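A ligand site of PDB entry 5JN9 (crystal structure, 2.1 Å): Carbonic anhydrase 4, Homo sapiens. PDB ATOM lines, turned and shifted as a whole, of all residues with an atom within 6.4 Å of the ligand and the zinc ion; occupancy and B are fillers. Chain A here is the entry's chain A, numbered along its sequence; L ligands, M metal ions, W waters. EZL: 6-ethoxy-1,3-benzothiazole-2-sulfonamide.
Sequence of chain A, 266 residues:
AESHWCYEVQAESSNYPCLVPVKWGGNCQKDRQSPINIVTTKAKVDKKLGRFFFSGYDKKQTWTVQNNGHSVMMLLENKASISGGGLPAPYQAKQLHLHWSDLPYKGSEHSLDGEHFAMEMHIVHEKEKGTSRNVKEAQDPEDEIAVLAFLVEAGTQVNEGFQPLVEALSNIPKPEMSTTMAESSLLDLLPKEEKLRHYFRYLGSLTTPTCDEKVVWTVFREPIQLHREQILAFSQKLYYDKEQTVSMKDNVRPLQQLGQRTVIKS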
ATOM      1  N   TYR A   7       3.256   8.166 -29.310  1.00  0.00           N
ATOM      2  CA  TYR A   7       3.265   8.801 -27.985  1.00  0.00           C
ATOM      3  C   TYR A   7       4.276   9.972 -27.967  1.00  0.00           C
ATOM      4  O   TYR A   7       5.176  10.083 -28.837  1.00  0.00           O
ATOM      5  CB  TYR A   7       3.615   7.789 -26.924  1.00  0.00           C
ATOM      6  CG  TYR A   7       2.613   6.668 -26.732  1.00  0.00           C
ATOM      7  CD1 TYR A   7       1.449   6.891 -26.028  1.00  0.00           C
ATOM      8  CD2 TYR A   7       2.855   5.391 -27.222  1.00  0.00           C
ATOM      9  CE1 TYR A   7       0.547   5.865 -25.799  1.00  0.00           C
ATOM     10  CE2 TYR A   7       1.957   4.355 -27.020  1.00  0.00           C
ATOM     11  CZ  TYR A   7       0.820   4.587 -26.315  1.00  0.00           C
ATOM     12  OH  TYR A   7      -0.035   3.583 -26.129  1.00  0.00           O
ATOM     13  N   GLN A  95      -6.559 -10.504 -25.982  1.00  0.00           N
ATOM     14  CA  GLN A  95      -5.180 -10.096 -25.840  1.00  0.00           C
ATOM     15  C   GLN A  95      -4.931  -9.398 -24.527  1.00  0.00           C
ATOM     16  O   GLN A  95      -5.842  -8.777 -23.964  1.00  0.00           O
ATOM     17  CB  GLN A  95      -4.735  -9.244 -27.014  1.00  0.00           C
ATOM     18  CG  GLN A  95      -5.611  -8.047 -27.299  1.00  0.00           C
ATOM     19  CD  GLN A  95      -4.933  -6.740 -26.969  1.00  0.00           C
ATOM     20  OE1 GLN A  95      -3.965  -6.698 -26.176  1.00  0.00           O
ATOM     21  NE2 GLN A  95      -5.424  -5.653 -27.587  1.00  0.00           N
ATOM     22  N   HIS A  97      -1.919  -6.745 -22.766  1.00  0.00           N
ATOM     23  CA  HIS A  97      -0.744  -5.898 -23.022  1.00  0.00           C
ATOM     24  C   HIS A  97      -0.482  -4.948 -21.884  1.00  0.00           C
ATOM     25  O   HIS A  97      -1.178  -4.980 -20.865  1.00  0.00           O
ATOM     26  CB  HIS A  97      -0.890  -5.153 -24.361  1.00  0.00           C
ATOM     27  CG  HIS A  97      -2.033  -4.204 -24.367  1.00  0.00           C
ATOM     28  ND1 HIS A  97      -3.287  -4.589 -24.744  1.00  0.00           N
ATOM     29  CD2 HIS A  97      -2.144  -2.925 -23.952  1.00  0.00           C
ATOM     30  CE1 HIS A  97      -4.135  -3.586 -24.598  1.00  0.00           C
ATOM     31  NE2 HIS A  97      -3.466  -2.562 -24.113  1.00  0.00           N
ATOM     32  N   LEU A  98       0.531  -4.104 -22.039  1.00  0.00           N
ATOM     33  CA  LEU A  98       0.943  -3.235 -20.941  1.00  0.00           C
ATOM     34  C   LEU A  98       1.342  -1.840 -21.393  1.00  0.00           C
ATOM     35  O   LEU A  98       1.623  -1.582 -22.545  1.00  0.00           O
ATOM     36  CB  LEU A  98       2.095  -3.883 -20.126  1.00  0.00           C
ATOM     37  CG  LEU A  98       1.742  -5.157 -19.343  1.00  0.00           C
ATOM     38  CD1 LEU A  98       2.094  -6.404 -20.115  1.00  0.00           C
ATOM     39  CD2 LEU A  98       2.465  -5.207 -17.990  1.00  0.00           C
ATOM     40  N   HIS A  99       1.325  -0.946 -20.424  1.00  0.00           N
ATOM     41  CA  HIS A  99       1.791   0.420 -20.573  1.00  0.00           C
ATOM     42  C   HIS A  99       2.705   0.622 -19.373  1.00  0.00           C
ATOM     43  O   HIS A  99       2.397   0.127 -18.291  1.00  0.00           O
ATOM     44  CB  HIS A  99       0.629   1.369 -20.485  1.00  0.00           C
ATOM     45  CG  HIS A  99      -0.426   1.115 -21.509  1.00  0.00           C
ATOM     46  ND1 HIS A  99      -0.465   1.789 -22.717  1.00  0.00           N
ATOM     47  CD2 HIS A  99      -1.483   0.273 -21.524  1.00  0.00           C
ATOM     48  CE1 HIS A  99      -1.505   1.377 -23.422  1.00  0.00           C
ATOM     49  NE2 HIS A  99      -2.117   0.455 -22.726  1.00  0.00           N
ATOM     50  N   GLU A 109      -1.845   4.246 -17.058  1.00  0.00           N
ATOM     51  CA  GLU A 109      -2.715   5.152 -17.818  1.00  0.00           C
ATOM     52  C   GLU A 109      -3.727   5.816 -16.901  1.00  0.00           C
ATOM     53  O   GLU A 109      -3.779   7.021 -16.826  1.00  0.00           O
ATOM     54  CB  GLU A 109      -3.385   4.438 -18.996  1.00  0.00           C
ATOM     55  CG  GLU A 109      -2.366   3.900 -20.000  1.00  0.00           C
ATOM     56  CD  GLU A 109      -2.908   3.827 -21.406  1.00  0.00           C
ATOM     57  OE1 GLU A 109      -3.787   2.960 -21.640  1.00  0.00           O
ATOM     58  OE2 GLU A 109      -2.445   4.639 -22.251  1.00  0.00           O
ATOM     59  N   GLU A 120       0.536  -0.261 -16.059  1.00  0.00           N
ATOM     60  CA  GLU A 120      -0.878  -0.688 -16.126  1.00  0.00           C
ATOM     61  C   GLU A 120      -0.970  -1.804 -17.142  1.00  0.00           C
ATOM     62  O   GLU A 120      -0.480  -1.678 -18.274  1.00  0.00           O
ATOM     63  CB  GLU A 120      -1.787   0.454 -16.558  1.00  0.00           C
ATOM     64  CG  GLU A 120      -3.270   0.159 -16.350  1.00  0.00           C
ATOM     65  CD  GLU A 120      -4.141   1.393 -16.399  1.00  0.00           C
ATOM     66  OE1 GLU A 120      -3.664   2.483 -15.973  1.00  0.00           O
ATOM     67  OE2 GLU A 120      -5.311   1.277 -16.868  1.00  0.00           O
ATOM     68  N   MET A 121      -1.578  -2.909 -16.735  1.00  0.00           N
ATOM     69  CA  MET A 121      -1.769  -4.085 -17.608  1.00  0.00           C
ATOM     70  C   MET A 121      -3.231  -4.149 -17.996  1.00  0.00           C
ATOM     71  O   MET A 121      -4.106  -4.075 -17.123  1.00  0.00           O
ATOM     72  CB  MET A 121      -1.396  -5.376 -16.851  1.00  0.00           C
ATOM     73  CG  MET A 121      -1.695  -6.698 -17.571  1.00  0.00           C
ATOM     74  SD  MET A 121      -0.885  -8.063 -16.678  1.00  0.00           S
ATOM     75  CE  MET A 121      -2.262  -8.423 -15.652  1.00  0.00           C
ATOM     76  N   HIS A 122      -3.475  -4.366 -19.287  1.00  0.00           N
ATOM     77  CA  HIS A 122      -4.811  -4.419 -19.861  1.00  0.00           C
ATOM     78  C   HIS A 122      -5.091  -5.770 -20.471  1.00  0.00           C
ATOM     79  O   HIS A 122      -4.329  -6.215 -21.339  1.00  0.00           O
ATOM     80  CB  HIS A 122      -4.946  -3.359 -20.913  1.00  0.00           C
ATOM     81  CG  HIS A 122      -5.010  -1.977 -20.365  1.00  0.00           C
ATOM     82  ND1 HIS A 122      -4.655  -0.870 -21.109  1.00  0.00           N
ATOM     83  CD2 HIS A 122      -5.304  -1.516 -19.128  1.00  0.00           C
ATOM     84  CE1 HIS A 122      -4.770   0.217 -20.367  1.00  0.00           C
ATOM     85  NE2 HIS A 122      -5.157  -0.155 -19.160  1.00  0.00           N
ATOM     86  N   ILE A 123      -6.200  -6.401 -20.055  1.00  0.00           N
ATOM     87  CA  ILE A 123      -6.661  -7.662 -20.654  1.00  0.00           C
ATOM     88  C   ILE A 123      -7.953  -7.316 -21.396  1.00  0.00           C
ATOM     89  O   ILE A 123      -8.928  -6.845 -20.780  1.00  0.00           O
ATOM     90  CB  ILE A 123      -6.868  -8.812 -19.631  1.00  0.00           C
ATOM     91  CG1 ILE A 123      -5.663  -8.980 -18.699  1.00  0.00           C
ATOM     92  CG2 ILE A 123      -7.043 -10.146 -20.358  1.00  0.00           C
ATOM     93  CD1 ILE A 123      -5.775 -10.141 -17.698  1.00  0.00           C
ATOM     94  N   VAL A 124      -7.929  -7.523 -22.718  1.00  0.00           N
ATOM     95  CA  VAL A 124      -8.933  -7.011 -23.609  1.00  0.00           C
ATOM     96  C   VAL A 124      -9.842  -8.167 -23.938  1.00  0.00           C
ATOM     97  O   VAL A 124      -9.384  -9.207 -24.409  1.00  0.00           O
ATOM     98  CB  VAL A 124      -8.300  -6.469 -24.908  1.00  0.00           C
ATOM     99  CG1 VAL A 124      -9.356  -5.924 -25.874  1.00  0.00           C
ATOM    100  CG2 VAL A 124      -7.241  -5.415 -24.614  1.00  0.00           C
ATOM    101  N   ILE A 145     -16.441  -4.089 -25.761  1.00  0.00           N
ATOM    102  CA  ILE A 145     -15.136  -4.476 -25.281  1.00  0.00           C
ATOM    103  C   ILE A 145     -15.120  -4.214 -23.800  1.00  0.00           C
ATOM    104  O   ILE A 145     -15.570  -3.151 -23.357  1.00  0.00           O
ATOM    105  CB  ILE A 145     -14.062  -3.657 -25.987  1.00  0.00           C
ATOM    106  CG1 ILE A 145     -14.138  -3.938 -27.484  1.00  0.00           C
ATOM    107  CG2 ILE A 145     -12.671  -3.977 -25.430  1.00  0.00           C
ATOM    108  CD1 ILE A 145     -13.291  -3.026 -28.307  1.00  0.00           C
ATOM    109  N   VAL A 147     -12.223  -4.149 -20.914  1.00  0.00           N
ATOM    110  CA  VAL A 147     -10.827  -4.190 -20.575  1.00  0.00           C
ATOM    111  C   VAL A 147     -10.742  -4.217 -19.074  1.00  0.00           C
ATOM    112  O   VAL A 147     -11.351  -3.383 -18.405  1.00  0.00           O
ATOM    113  CB  VAL A 147     -10.016  -2.964 -21.076  1.00  0.00           C
ATOM    114  CG1 VAL A 147      -8.563  -3.042 -20.584  1.00  0.00           C
ATOM    115  CG2 VAL A 147     -10.085  -2.829 -22.580  1.00  0.00           C
ATOM    116  N   SER A 205     -13.330   4.647 -23.592  1.00  0.00           N
ATOM    117  CA  SER A 205     -12.733   4.379 -24.887  1.00  0.00           C
ATOM    118  C   SER A 205     -11.512   3.474 -24.818  1.00  0.00           C
ATOM    119  O   SER A 205     -10.968   3.164 -23.759  1.00  0.00           O
ATOM    120  CB  SER A 205     -12.331   5.688 -25.566  1.00  0.00           C
ATOM    121  OG  SER A 205     -11.095   6.179 -25.091  1.00  0.00           O
ATOM    122  N   LEU A 206     -11.069   3.074 -26.007  1.00  0.00           N
ATOM    123  CA  LEU A 206      -9.777   2.461 -26.192  1.00  0.00           C
ATOM    124  C   LEU A 206      -8.750   3.627 -26.029  1.00  0.00           C
ATOM    125  O   LEU A 206      -9.073   4.766 -26.324  1.00  0.00           O
ATOM    126  CB  LEU A 206      -9.725   1.813 -27.577  1.00  0.00           C
ATOM    127  CG  LEU A 206     -10.712   0.659 -27.877  1.00  0.00           C
ATOM    128  CD1 LEU A 206     -10.763   0.346 -29.358  1.00  0.00           C
ATOM    129  CD2 LEU A 206     -10.342  -0.585 -27.084  1.00  0.00           C
ATOM    130  N   THR A 207      -7.579   3.334 -25.467  1.00  0.00           N
ATOM    131  CA  THR A 207      -6.558   4.347 -25.186  1.00  0.00           C
ATOM    132  C   THR A 207      -5.512   4.551 -26.290  1.00  0.00           C
ATOM    133  O   THR A 207      -4.659   5.472 -26.177  1.00  0.00           O
ATOM    134  CB  THR A 207      -5.828   4.080 -23.839  1.00  0.00           C
ATOM    135  OG1 THR A 207      -5.095   2.852 -23.881  1.00  0.00           O
ATOM    136  CG2 THR A 207      -6.835   4.057 -22.674  1.00  0.00           C
ATOM    137  N   THR A 208      -5.550   3.717 -27.322  1.00  0.00           N
ATOM    138  CA  THR A 208      -4.780   3.981 -28.551  1.00  0.00           C
ATOM    139  C   THR A 208      -5.727   4.116 -29.738  1.00  0.00           C
ATOM    140  O   THR A 208      -6.866   3.649 -29.655  1.00  0.00           O
ATOM    141  CB  THR A 208      -3.705   2.921 -28.797  1.00  0.00           C
ATOM    142  OG1 THR A 208      -4.313   1.646 -28.954  1.00  0.00           O
ATOM    143  CG2 THR A 208      -2.727   2.873 -27.615  1.00  0.00           C
ATOM    144  N   PRO A 209      -5.302   4.793 -30.821  1.00  0.00           N
ATOM    145  CA  PRO A 209      -6.240   4.998 -31.945  1.00  0.00           C
ATOM    146  C   PRO A 209      -6.715   3.711 -32.538  1.00  0.00           C
ATOM    147  O   PRO A 209      -5.913   2.781 -32.589  1.00  0.00           O
ATOM    148  CB  PRO A 209      -5.429   5.784 -32.967  1.00  0.00           C
ATOM    149  CG  PRO A 209      -4.381   6.504 -32.144  1.00  0.00           C
ATOM    150  CD  PRO A 209      -4.022   5.507 -31.054  1.00  0.00           C
ATOM    151  N   THR A 210      -7.966   3.631 -32.991  1.00  0.00           N
ATOM    152  CA  THR A 210      -8.895   4.751 -33.192  1.00  0.00           C
ATOM    153  C   THR A 210      -9.781   5.171 -31.961  1.00  0.00           C
ATOM    154  O   THR A 210     -10.773   5.858 -32.115  1.00  0.00           O
ATOM    155  CB  THR A 210      -9.833   4.430 -34.408  1.00  0.00           C
ATOM    156  OG1 THR A 210     -10.545   3.201 -34.201  1.00  0.00           O
ATOM    157  CG2 THR A 210      -9.068   4.318 -35.653  1.00  0.00           C
ATOM    158  N   CYS A 211      -9.410   4.772 -30.749  1.00  0.00           N
ATOM    159  CA  CYS A 211     -10.019   5.322 -29.515  1.00  0.00           C
ATOM    160  C   CYS A 211     -11.542   5.188 -29.447  1.00  0.00           C
ATOM    161  O   CYS A 211     -12.261   6.101 -29.020  1.00  0.00           O
ATOM    162  CB  CYS A 211      -9.637   6.790 -29.317  1.00  0.00           C
ATOM    163  SG  CYS A 211      -7.847   7.168 -29.370  1.00  0.00           S
ATOM    164  N   VAL A 215     -15.867   0.754 -24.726  1.00  0.00           N
ATOM    165  CA  VAL A 215     -15.223  -0.017 -23.698  1.00  0.00           C
ATOM    166  C   VAL A 215     -15.931   0.132 -22.370  1.00  0.00           C
ATOM    167  O   VAL A 215     -16.188   1.238 -21.897  1.00  0.00           O
ATOM    168  CB  VAL A 215     -13.752   0.404 -23.534  1.00  0.00           C
ATOM    169  CG1 VAL A 215     -13.097  -0.376 -22.383  1.00  0.00           C
ATOM    170  CG2 VAL A 215     -13.007   0.190 -24.854  1.00  0.00           C
ATOM    171  N   TRP A 217     -14.878  -0.343 -18.780  1.00  0.00           N
ATOM    172  CA  TRP A 217     -13.635  -0.377 -18.018  1.00  0.00           C
ATOM    173  C   TRP A 217     -13.831  -0.944 -16.620  1.00  0.00           C
ATOM    174  O   TRP A 217     -14.810  -0.603 -15.927  1.00  0.00           O
ATOM    175  CB  TRP A 217     -13.031   1.023 -17.885  1.00  0.00           C
ATOM    176  CG  TRP A 217     -12.276   1.389 -19.067  1.00  0.00           C
ATOM    177  CD1 TRP A 217     -12.712   2.165 -20.091  1.00  0.00           C
ATOM    178  CD2 TRP A 217     -10.962   0.954 -19.419  1.00  0.00           C
ATOM    179  NE1 TRP A 217     -11.745   2.249 -21.058  1.00  0.00           N
ATOM    180  CE2 TRP A 217     -10.648   1.523 -20.656  1.00  0.00           C
ATOM    181  CE3 TRP A 217      -9.994   0.151 -18.775  1.00  0.00           C
ATOM    182  CZ2 TRP A 217      -9.430   1.307 -21.309  1.00  0.00           C
ATOM    183  CZ3 TRP A 217      -8.774  -0.031 -19.386  1.00  0.00           C
ATOM    184  CH2 TRP A 217      -8.494   0.550 -20.644  1.00  0.00           C
HETATM  185  N1  EZL L   1      -5.199   0.350 -24.456  1.00  0.00           N
HETATM  186  C2  EZL L   1      -6.841  -0.346 -28.388  1.00  0.00           C
HETATM  187  C3  EZL L   1      -7.025  -1.802 -28.307  1.00  0.00           C
HETATM  188  C4  EZL L   1      -7.232  -2.540 -29.459  1.00  0.00           C
HETATM  189  C5  EZL L   1      -7.228  -1.897 -30.701  1.00  0.00           C
HETATM  190  C8  EZL L   1      -7.045  -3.923 -32.118  1.00  0.00           C
HETATM  191  O1  EZL L   1      -6.695  -1.651 -23.788  1.00  0.00           O
HETATM  192  O2  EZL L   1      -7.563   0.478 -24.202  1.00  0.00           O
HETATM  193  S1  EZL L   1      -6.557  -0.466 -24.599  1.00  0.00           S
HETATM  194  C1  EZL L   1      -6.730  -0.840 -26.208  1.00  0.00           C
HETATM  195  N2  EZL L   1      -6.661   0.129 -27.137  1.00  0.00           N
HETATM  196  S2  EZL L   1      -7.027  -2.474 -26.774  1.00  0.00           S
HETATM  197  C6  EZL L   1      -7.039  -0.518 -30.797  1.00  0.00           C
HETATM  198  C7  EZL L   1      -6.853   0.240 -29.657  1.00  0.00           C
HETATM  199  O3  EZL L   1      -7.422  -2.558 -31.888  1.00  0.00           O
HETATM  200  C9  EZL L   1      -6.265  -4.022 -33.419  1.00  0.00           C
HETATM  201 ZN    ZN M   1      -3.903  -0.641 -23.136  1.00  0.00          ZN
HETATM  202  O   HOH W   1      -3.688  -2.843 -28.146  1.00  0.00           O
HETATM  203  O   HOH W   2      -3.681  -0.375 -27.232  1.00  0.00           O
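The backbone NH (N) of Thr 207 is in hydrogen-bond range of an oxygen (O2) of the ligand (3.1 Å).
OG1 of Thr 207 lies within hydrogen-bond range of O2 of the ligand (3.4 Å).
A nitrogen (N2) of the ligand lies close to the side-chain hydroxyl (OG1) of Thr 208 (3.3 Å).
The side-chain amide nitrogen of Gln 95 sits close to a sulfur (S2) of the ligand, 3.7 Å away.
Water W2 lies within hydrogen-bond range of OG1 of Thr 208 (2.7 Å) and N2 of the ligand (3.0 Å).
Water W1 lies within hydrogen-bond range of the side-chain amide nitrogen (NE2) of Gln 95 and a sulfur (S2) of the ligand.
The zinc ion is bound by a nitrogen (N1) of the ligand (2.1 Å), a ring nitrogen (NE2) of His 99 (2.1 Å), a ring nitrogen (ND1) of His 122 (2.2 Å) and a ring nitrogen (NE2) of His 97 (2.2 Å).
The zinc ion has four donor atoms within binding distance.
Merely in contact with the ligand: Leu 206 (3.5 Å), Trp 217 (3.5 Å), Val 124 (3.7 Å), Val 147 (3.8 Å) and Pro 209 (3.9 Å).
Hydrophobic or aromatic side chains that line the ligand: His 97, His 99, His 122, Val 124, Val 147, Leu 206 and Trp 217.
11 residues have an atom within 4 Å of the ligand: Gln 95, His 97, His 99, His 122, Val 124, Val 147, Leu 206, Thr 207, Thr 208, Pro 209 and Trp 217.
The nearest printed residue that does not touch the ligand is Glu 109 (4.1 Å).
OE1 of Glu 109 touches the zinc ion (3.9 Å).
OG1 of Thr 207 touches the zinc ion, 3.8 Å away.
Along chain A the residues within 4 Å of the zinc ion span positions 97 to 207.
A ring nitrogen (NE2) of His 99 lies close to the side-chain carboxylate of Glu 109, at 3.2 Å.
N of His 99 is in hydrogen-bond range of O of Glu 120 (2.9 Å).
A ring nitrogen (NE2) of His 122 is in hydrogen-bond range of the side-chain carboxylate (OE2) of Glu 120.
The side-chain amide oxygen (OE1) of Gln 95 sits at hydrogen-bond distance from a ring nitrogen (ND1) of His 97 (2.6 Å).
OG1 of Thr 207 sits at hydrogen-bond distance from OE1 of Glu 109 (2.6 Å).
The backbone carbonyl oxygen of Ser 205 lies within hydrogen-bond range of the indole nitrogen of Trp 217, at 3.0 Å.
The backbone carbonyl oxygen (O) of Gln 95 lies within hydrogen-bond range of the backbone NH (N) of Val 124 (2.7 Å).
N of Glu 109 sits at hydrogen-bond distance from OE1 of Glu 120.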
